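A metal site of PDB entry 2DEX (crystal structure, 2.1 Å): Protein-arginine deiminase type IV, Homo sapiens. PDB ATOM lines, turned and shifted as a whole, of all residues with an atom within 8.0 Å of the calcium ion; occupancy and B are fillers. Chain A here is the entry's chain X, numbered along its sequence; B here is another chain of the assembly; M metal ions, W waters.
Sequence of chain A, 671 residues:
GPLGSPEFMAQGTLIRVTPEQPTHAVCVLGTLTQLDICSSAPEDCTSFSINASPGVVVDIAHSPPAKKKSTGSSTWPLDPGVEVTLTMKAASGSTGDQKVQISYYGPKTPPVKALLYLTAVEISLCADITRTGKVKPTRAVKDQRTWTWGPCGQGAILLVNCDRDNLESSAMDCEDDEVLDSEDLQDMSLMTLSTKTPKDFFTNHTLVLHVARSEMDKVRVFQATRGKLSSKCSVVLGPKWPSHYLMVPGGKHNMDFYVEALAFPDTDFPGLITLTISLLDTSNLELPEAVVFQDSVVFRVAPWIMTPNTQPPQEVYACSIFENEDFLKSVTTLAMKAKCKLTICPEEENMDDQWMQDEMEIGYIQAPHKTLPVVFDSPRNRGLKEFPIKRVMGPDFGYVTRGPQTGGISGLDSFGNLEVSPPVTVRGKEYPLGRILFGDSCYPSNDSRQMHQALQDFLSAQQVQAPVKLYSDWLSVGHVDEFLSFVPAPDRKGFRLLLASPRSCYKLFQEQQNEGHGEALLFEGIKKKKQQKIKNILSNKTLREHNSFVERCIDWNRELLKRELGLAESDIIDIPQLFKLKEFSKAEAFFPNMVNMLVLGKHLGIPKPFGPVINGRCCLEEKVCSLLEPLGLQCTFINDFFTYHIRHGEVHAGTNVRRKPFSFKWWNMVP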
ATOM      1  N   MET A 306     -14.647   0.942   0.609  1.00  0.00           N
ATOM      2  CA  MET A 306     -14.575   2.281  -0.012  1.00  0.00           C
ATOM      3  C   MET A 306     -15.939   2.926   0.043  1.00  0.00           C
ATOM      4  O   MET A 306     -16.936   2.224   0.216  1.00  0.00           O
ATOM      5  CB  MET A 306     -14.152   2.154  -1.487  1.00  0.00           C
ATOM      6  CG  MET A 306     -12.694   1.982  -1.705  1.00  0.00           C
ATOM      7  SD  MET A 306     -12.216   1.828  -3.452  1.00  0.00           S
ATOM      8  CE  MET A 306     -12.647   3.464  -3.992  1.00  0.00           C
ATOM      9  N   THR A 307     -15.974   4.244  -0.151  1.00  0.00           N
ATOM     10  CA  THR A 307     -17.223   5.034  -0.136  1.00  0.00           C
ATOM     11  C   THR A 307     -17.440   5.807  -1.437  1.00  0.00           C
ATOM     12  O   THR A 307     -16.622   6.648  -1.781  1.00  0.00           O
ATOM     13  CB  THR A 307     -17.195   6.061   1.001  1.00  0.00           C
ATOM     14  OG1 THR A 307     -15.949   6.793   0.929  1.00  0.00           O
ATOM     15  CG2 THR A 307     -17.309   5.369   2.355  1.00  0.00           C
ATOM     16  N   ASN A 309     -19.302   8.400  -4.303  1.00  0.00           N
ATOM     17  CA  ASN A 309     -19.583   9.832  -4.320  1.00  0.00           C
ATOM     18  C   ASN A 309     -20.960  10.164  -3.739  1.00  0.00           C
ATOM     19  O   ASN A 309     -21.209  11.319  -3.444  1.00  0.00           O
ATOM     20  CB  ASN A 309     -19.491  10.375  -5.750  1.00  0.00           C
ATOM     21  CG  ASN A 309     -18.049  10.445  -6.240  1.00  0.00           C
ATOM     22  OD1 ASN A 309     -17.103  10.228  -5.488  1.00  0.00           O
ATOM     23  ND2 ASN A 309     -17.881  10.749  -7.518  1.00  0.00           N
ATOM     24  N   MET A 356      -3.645  15.103  -5.330  1.00  0.00           N
ATOM     25  CA  MET A 356      -4.128  14.585  -4.046  1.00  0.00           C
ATOM     26  C   MET A 356      -5.031  13.335  -4.211  1.00  0.00           C
ATOM     27  O   MET A 356      -5.081  12.464  -3.323  1.00  0.00           O
ATOM     28  CB  MET A 356      -4.832  15.716  -3.259  1.00  0.00           C
ATOM     29  CG  MET A 356      -5.299  15.380  -1.845  1.00  0.00           C
ATOM     30  SD  MET A 356      -4.033  14.710  -0.748  1.00  0.00           S
ATOM     31  CE  MET A 356      -3.295  16.184  -0.083  1.00  0.00           C
ATOM     32  N   GLN A 357      -5.699  13.215  -5.364  1.00  0.00           N
ATOM     33  CA  GLN A 357      -6.505  12.045  -5.719  1.00  0.00           C
ATOM     34  C   GLN A 357      -5.730  10.744  -5.827  1.00  0.00           C
ATOM     35  O   GLN A 357      -6.255   9.648  -5.555  1.00  0.00           O
ATOM     36  CB  GLN A 357      -7.224  12.299  -7.050  1.00  0.00           C
ATOM     37  CG  GLN A 357      -8.053  11.143  -7.623  1.00  0.00           C
ATOM     38  CD  GLN A 357      -9.272  10.807  -6.755  1.00  0.00           C
ATOM     39  OE1 GLN A 357      -9.802   9.681  -6.804  1.00  0.00           O
ATOM     40  NE2 GLN A 357      -9.689  11.765  -5.913  1.00  0.00           N
ATOM     41  N   ASP A 358      -4.474  10.836  -6.242  1.00  0.00           N
ATOM     42  CA  ASP A 358      -3.787   9.681  -6.803  1.00  0.00           C
ATOM     43  C   ASP A 358      -3.024   8.820  -5.795  1.00  0.00           C
ATOM     44  O   ASP A 358      -2.926   7.605  -5.952  1.00  0.00           O
ATOM     45  CB  ASP A 358      -2.886  10.141  -7.955  1.00  0.00           C
ATOM     46  CG  ASP A 358      -3.672  10.590  -9.177  1.00  0.00           C
ATOM     47  OD1 ASP A 358      -4.867  10.187  -9.340  1.00  0.00           O
ATOM     48  OD2 ASP A 358      -3.131  11.393  -9.954  1.00  0.00           O
ATOM     49  N   MET A 360      -3.726   8.261  -2.610  1.00  0.00           N
ATOM     50  CA  MET A 360      -4.513   7.576  -1.580  1.00  0.00           C
ATOM     51  C   MET A 360      -6.018   7.465  -1.837  1.00  0.00           C
ATOM     52  O   MET A 360      -6.591   8.184  -2.664  1.00  0.00           O
ATOM     53  CB  MET A 360      -4.334   8.289  -0.260  1.00  0.00           C
ATOM     54  CG  MET A 360      -5.079   9.588  -0.187  1.00  0.00           C
ATOM     55  SD  MET A 360      -4.768  10.467   1.334  1.00  0.00           S
ATOM     56  CE  MET A 360      -5.938  11.805   1.151  1.00  0.00           C
ATOM     57  N   GLU A 361      -6.628   6.544  -1.099  1.00  0.00           N
ATOM     58  CA  GLU A 361      -8.061   6.369  -1.097  1.00  0.00           C
ATOM     59  C   GLU A 361      -8.452   6.169   0.341  1.00  0.00           C
ATOM     60  O   GLU A 361      -7.893   5.311   1.011  1.00  0.00           O
ATOM     61  CB  GLU A 361      -8.461   5.154  -1.957  1.00  0.00           C
ATOM     62  CG  GLU A 361      -9.941   4.910  -2.137  1.00  0.00           C
ATOM     63  CD  GLU A 361     -10.665   5.889  -3.093  1.00  0.00           C
ATOM     64  OE1 GLU A 361     -10.140   6.240  -4.175  1.00  0.00           O
ATOM     65  OE2 GLU A 361     -11.816   6.271  -2.787  1.00  0.00           O
ATOM     66  N   ILE A 362      -9.423   6.940   0.800  1.00  0.00           N
ATOM     67  CA  ILE A 362      -9.899   6.867   2.173  1.00  0.00           C
ATOM     68  C   ILE A 362     -11.128   5.993   2.170  1.00  0.00           C
ATOM     69  O   ILE A 362     -12.153   6.359   1.586  1.00  0.00           O
ATOM     70  CB  ILE A 362     -10.271   8.236   2.759  1.00  0.00           C
ATOM     71  CG1 ILE A 362      -9.209   9.296   2.447  1.00  0.00           C
ATOM     72  CG2 ILE A 362     -10.528   8.136   4.257  1.00  0.00           C
ATOM     73  CD1 ILE A 362      -7.846   8.923   2.792  1.00  0.00           C
ATOM     74  N   SER A 414      -2.192   4.661  -9.688  1.00  0.00           N
ATOM     75  CA  SER A 414      -2.658   5.936  -9.131  1.00  0.00           C
ATOM     76  C   SER A 414      -4.155   5.833  -8.809  1.00  0.00           C
ATOM     77  O   SER A 414      -4.924   5.277  -9.582  1.00  0.00           O
ATOM     78  CB  SER A 414      -2.410   7.049 -10.125  1.00  0.00           C
ATOM     79  OG  SER A 414      -1.030   7.291 -10.270  1.00  0.00           O
ATOM     80  N   PHE A 415      -4.572   6.361  -7.666  1.00  0.00           N
ATOM     81  CA  PHE A 415      -5.919   6.055  -7.195  1.00  0.00           C
ATOM     82  C   PHE A 415      -7.041   6.931  -7.766  1.00  0.00           C
ATOM     83  O   PHE A 415      -8.202   6.824  -7.351  1.00  0.00           O
ATOM     84  CB  PHE A 415      -5.930   5.945  -5.664  1.00  0.00           C
ATOM     85  CG  PHE A 415      -5.311   4.660  -5.125  1.00  0.00           C
ATOM     86  CD1 PHE A 415      -5.089   4.502  -3.778  1.00  0.00           C
ATOM     87  CD2 PHE A 415      -4.947   3.603  -5.989  1.00  0.00           C
ATOM     88  CE1 PHE A 415      -4.531   3.327  -3.246  1.00  0.00           C
ATOM     89  CE2 PHE A 415      -4.407   2.417  -5.493  1.00  0.00           C
ATOM     90  CZ  PHE A 415      -4.181   2.290  -4.113  1.00  0.00           C
ATOM     91  N   GLY A 416      -6.700   7.768  -8.762  1.00  0.00           N
ATOM     92  CA  GLY A 416      -7.694   8.292  -9.685  1.00  0.00           C
ATOM     93  C   GLY A 416      -8.325   7.171 -10.505  1.00  0.00           C
ATOM     94  O   GLY A 416      -9.412   7.323 -11.101  1.00  0.00           O
ATOM     95  N   ASN A 417      -7.612   6.038 -10.546  1.00  0.00           N
ATOM     96  CA  ASN A 417      -8.077   4.842 -11.202  1.00  0.00           C
ATOM     97  C   ASN A 417      -8.760   3.878 -10.272  1.00  0.00           C
ATOM     98  O   ASN A 417      -9.011   2.733 -10.646  1.00  0.00           O
ATOM     99  CB  ASN A 417      -6.915   4.136 -11.907  1.00  0.00           C
ATOM    100  CG  ASN A 417      -7.377   3.145 -12.957  1.00  0.00           C
ATOM    101  OD1 ASN A 417      -8.366   3.372 -13.670  1.00  0.00           O
ATOM    102  ND2 ASN A 417      -6.676   2.023 -13.057  1.00  0.00           N
ATOM    103  N   LEU A 418      -9.084   4.343  -9.063  1.00  0.00           N
ATOM    104  CA  LEU A 418      -9.761   3.507  -8.096  1.00  0.00           C
ATOM    105  C   LEU A 418     -11.001   4.247  -7.577  1.00  0.00           C
ATOM    106  O   LEU A 418     -10.892   5.278  -6.893  1.00  0.00           O
ATOM    107  CB  LEU A 418      -8.801   3.164  -6.954  1.00  0.00           C
ATOM    108  CG  LEU A 418      -9.390   2.342  -5.807  1.00  0.00           C
ATOM    109  CD1 LEU A 418      -9.915   1.033  -6.341  1.00  0.00           C
ATOM    110  CD2 LEU A 418      -8.399   2.101  -4.715  1.00  0.00           C
ATOM    111  N   GLU A 419     -12.162   3.714  -7.897  1.00  0.00           N
ATOM    112  CA  GLU A 419     -13.456   4.316  -7.553  1.00  0.00           C
ATOM    113  C   GLU A 419     -14.429   3.216  -7.123  1.00  0.00           C
ATOM    114  O   GLU A 419     -14.072   2.030  -7.116  1.00  0.00           O
ATOM    115  CB  GLU A 419     -14.027   5.078  -8.748  1.00  0.00           C
ATOM    116  CG  GLU A 419     -13.143   6.215  -9.319  1.00  0.00           C
ATOM    117  CD  GLU A 419     -12.858   7.341  -8.313  1.00  0.00           C
ATOM    118  OE1 GLU A 419     -11.670   7.783  -8.167  1.00  0.00           O
ATOM    119  OE2 GLU A 419     -13.814   7.762  -7.642  1.00  0.00           O
ATOM    120  N   VAL A 420     -15.644   3.608  -6.734  1.00  0.00           N
ATOM    121  CA  VAL A 420     -16.675   2.655  -6.289  1.00  0.00           C
ATOM    122  C   VAL A 420     -18.084   3.163  -6.666  1.00  0.00           C
ATOM    123  O   VAL A 420     -18.386   4.383  -6.621  1.00  0.00           O
ATOM    124  CB  VAL A 420     -16.514   2.336  -4.751  1.00  0.00           C
ATOM    125  CG1 VAL A 420     -16.613   3.549  -3.879  1.00  0.00           C
ATOM    126  CG2 VAL A 420     -17.500   1.303  -4.274  1.00  0.00           C
ATOM    127  N   LEU A 437     -14.652  -0.167  -8.850  1.00  0.00           N
ATOM    128  CA  LEU A 437     -14.414   0.036 -10.256  1.00  0.00           C
ATOM    129  C   LEU A 437     -12.971   0.476 -10.406  1.00  0.00           C
ATOM    130  O   LEU A 437     -12.570   1.475  -9.776  1.00  0.00           O
ATOM    131  CB  LEU A 437     -15.257   1.208 -10.725  1.00  0.00           C
ATOM    132  CG  LEU A 437     -16.717   1.079 -11.196  1.00  0.00           C
ATOM    133  CD1 LEU A 437     -17.378  -0.166 -10.884  1.00  0.00           C
ATOM    134  CD2 LEU A 437     -17.518   2.292 -10.756  1.00  0.00           C
ATOM    135  N   VAL A 480     -10.126   5.738 -14.586  1.00  0.00           N
ATOM    136  CA  VAL A 480     -11.583   5.748 -14.738  1.00  0.00           C
ATOM    137  C   VAL A 480     -12.218   7.111 -14.436  1.00  0.00           C
ATOM    138  O   VAL A 480     -13.217   7.444 -15.035  1.00  0.00           O
ATOM    139  CB  VAL A 480     -12.285   4.612 -13.967  1.00  0.00           C
ATOM    140  CG1 VAL A 480     -11.896   3.260 -14.558  1.00  0.00           C
ATOM    141  CG2 VAL A 480     -11.991   4.662 -12.473  1.00  0.00           C
ATOM    142  N   ASP A 481     -11.607   7.910 -13.552  1.00  0.00           N
ATOM    143  CA  ASP A 481     -12.142   9.225 -13.189  1.00  0.00           C
ATOM    144  C   ASP A 481     -12.038  10.239 -14.339  1.00  0.00           C
ATOM    145  O   ASP A 481     -12.620  11.327 -14.259  1.00  0.00           O
ATOM    146  CB  ASP A 481     -11.555   9.718 -11.829  1.00  0.00           C
ATOM    147  CG  ASP A 481     -10.162  10.375 -11.918  1.00  0.00           C
ATOM    148  OD1 ASP A 481      -9.800  11.088 -10.931  1.00  0.00           O
ATOM    149  OD2 ASP A 481      -9.429  10.215 -12.925  1.00  0.00           O
ATOM    150  N   HIS A 652     -11.155  16.784  -9.693  1.00  0.00           N
ATOM    151  CA  HIS A 652     -11.158  15.506  -8.968  1.00  0.00           C
ATOM    152  C   HIS A 652      -9.742  15.018  -8.755  1.00  0.00           C
ATOM    153  O   HIS A 652      -9.398  14.537  -7.696  1.00  0.00           O
ATOM    154  CB  HIS A 652     -11.975  14.450  -9.741  1.00  0.00           C
ATOM    155  CG  HIS A 652     -12.268  13.201  -8.953  1.00  0.00           C
ATOM    156  ND1 HIS A 652     -11.652  11.991  -9.209  1.00  0.00           N
ATOM    157  CD2 HIS A 652     -13.143  12.977  -7.950  1.00  0.00           C
ATOM    158  CE1 HIS A 652     -12.122  11.084  -8.379  1.00  0.00           C
ATOM    159  NE2 HIS A 652     -13.015  11.657  -7.592  1.00  0.00           N
ATOM    160  N   THR A 655      -7.839  16.774  -5.780  1.00  0.00           N
ATOM    161  CA  THR A 655      -8.500  16.714  -4.474  1.00  0.00           C
ATOM    162  C   THR A 655      -8.784  15.253  -4.065  1.00  0.00           C
ATOM    163  O   THR A 655      -8.567  14.329  -4.839  1.00  0.00           O
ATOM    164  CB  THR A 655      -9.847  17.480  -4.472  1.00  0.00           C
ATOM    165  OG1 THR A 655     -10.745  16.909  -5.443  1.00  0.00           O
ATOM    166  CG2 THR A 655      -9.644  18.992  -4.771  1.00  0.00           C
ATOM    167  N   ASN A 656      -9.212  15.089  -2.825  1.00  0.00           N
ATOM    168  CA  ASN A 656      -9.647  13.784  -2.305  1.00  0.00           C
ATOM    169  C   ASN A 656     -10.688  14.060  -1.212  1.00  0.00           C
ATOM    170  O   ASN A 656     -10.802  15.196  -0.742  1.00  0.00           O
ATOM    171  CB  ASN A 656      -8.466  12.970  -1.780  1.00  0.00           C
ATOM    172  CG  ASN A 656      -8.585  11.504  -2.100  1.00  0.00           C
ATOM    173  OD1 ASN A 656      -9.678  10.935  -2.064  1.00  0.00           O
ATOM    174  ND2 ASN A 656      -7.459  10.880  -2.441  1.00  0.00           N
ATOM    175  N   VAL A 657     -11.463  13.044  -0.873  1.00  0.00           N
ATOM    176  CA  VAL A 657     -12.570  13.188   0.048  1.00  0.00           C
ATOM    177  C   VAL A 657     -12.722  11.943   0.923  1.00  0.00           C
ATOM    178  O   VAL A 657     -12.648  10.803   0.443  1.00  0.00           O
ATOM    179  CB  VAL A 657     -13.910  13.446  -0.694  1.00  0.00           C
ATOM    180  CG1 VAL A 657     -15.046  13.792   0.282  1.00  0.00           C
ATOM    181  CG2 VAL A 657     -13.738  14.580  -1.696  1.00  0.00           C
ATOM    182  N   ARG A 659     -15.545  10.180   3.276  1.00  0.00           N
ATOM    183  CA  ARG A 659     -16.994  10.198   3.276  1.00  0.00           C
ATOM    184  C   ARG A 659     -17.531   9.269   4.358  1.00  0.00           C
ATOM    185  O   ARG A 659     -16.822   8.370   4.842  1.00  0.00           O
ATOM    186  CB  ARG A 659     -17.544   9.776   1.918  1.00  0.00           C
ATOM    187  CG  ARG A 659     -16.969  10.566   0.739  1.00  0.00           C
ATOM    188  CD  ARG A 659     -17.560  10.144  -0.583  1.00  0.00           C
ATOM    189  NE  ARG A 659     -17.621  11.280  -1.506  1.00  0.00           N
ATOM    190  CZ  ARG A 659     -16.710  11.578  -2.430  1.00  0.00           C
ATOM    191  NH1 ARG A 659     -15.637  10.804  -2.631  1.00  0.00           N
ATOM    192  NH2 ARG A 659     -16.894  12.660  -3.161  1.00  0.00           N
ATOM    193  N   ARG B   4       0.219  14.527 -14.347  1.00  0.00           N
ATOM    194  CA  ARG B   4      -0.507  13.466 -13.642  1.00  0.00           C
ATOM    195  C   ARG B   4       0.012  12.069 -14.024  1.00  0.00           C
ATOM    196  O   ARG B   4      -0.049  11.150 -13.216  1.00  0.00           O
ATOM    197  CB  ARG B   4      -2.023  13.571 -13.873  1.00  0.00           C
ATOM    198  CG  ARG B   4      -2.823  12.740 -12.864  1.00  0.00           C
ATOM    199  CD  ARG B   4      -4.306  12.828 -13.092  1.00  0.00           C
ATOM    200  NE  ARG B   4      -5.053  12.257 -11.970  1.00  0.00           N
ATOM    201  CZ  ARG B   4      -6.330  11.849 -12.022  1.00  0.00           C
ATOM    202  NH1 ARG B   4      -7.026  11.932 -13.151  1.00  0.00           N
ATOM    203  NH2 ARG B   4      -6.901  11.367 -10.932  1.00  0.00           N
HETATM  204 CA    CA M   1     -10.135   7.460  -6.224  1.00  0.00          CA
HETATM  205  O   HOH W   1      -8.327   8.440  -4.790  1.00  0.00           O
HETATM  206  O   HOH W   2     -12.152   8.056  -4.945  1.00  0.00           O
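The backbone carbonyl oxygen (O) of Thr 655 sits at hydrogen-bond distance from the side-chain amide nitrogen (NE2) of Gln 357 (3.0 Å).
NE2 of Gln 357 sits close to O of His 652, 3.3 Å away.
The backbone carbonyl oxygen (O) of Glu 419 lies within hydrogen-bond range of the backbone NH (N) of Leu 437 (2.9 Å).
N of Phe 415 is in hydrogen-bond range of O of Asp 358 (2.7 Å).
Within 4 Å of the calcium ion: Gln 357, Glu 361, Phe 415, Leu 418 and Glu 419.
Along chain A the residues within 4 Å of the calcium ion span positions 357 to 419.
The calcium ion is bound by the side-chain amide oxygen (OE1) of Gln 357 (2.3 Å), the backbone carbonyl oxygen (O) of Phe 415 (2.3 Å), the side-chain carboxylate (OE1) of Glu 361 (2.4 Å), the backbone carbonyl oxygen (O) of Leu 418 (2.4 Å), water W2 (2.5 Å), the side-chain carboxylate (OE1) of Glu 419 (2.5 Å) and water W1 (2.5 Å).
Water W2 lies within hydrogen-bond range of OE2 of Glu 361 and OE2 of Glu 419.
Water W1 lies within hydrogen-bond range of O of Gln 357, O of Met 360 and ND2 of Asn 656.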
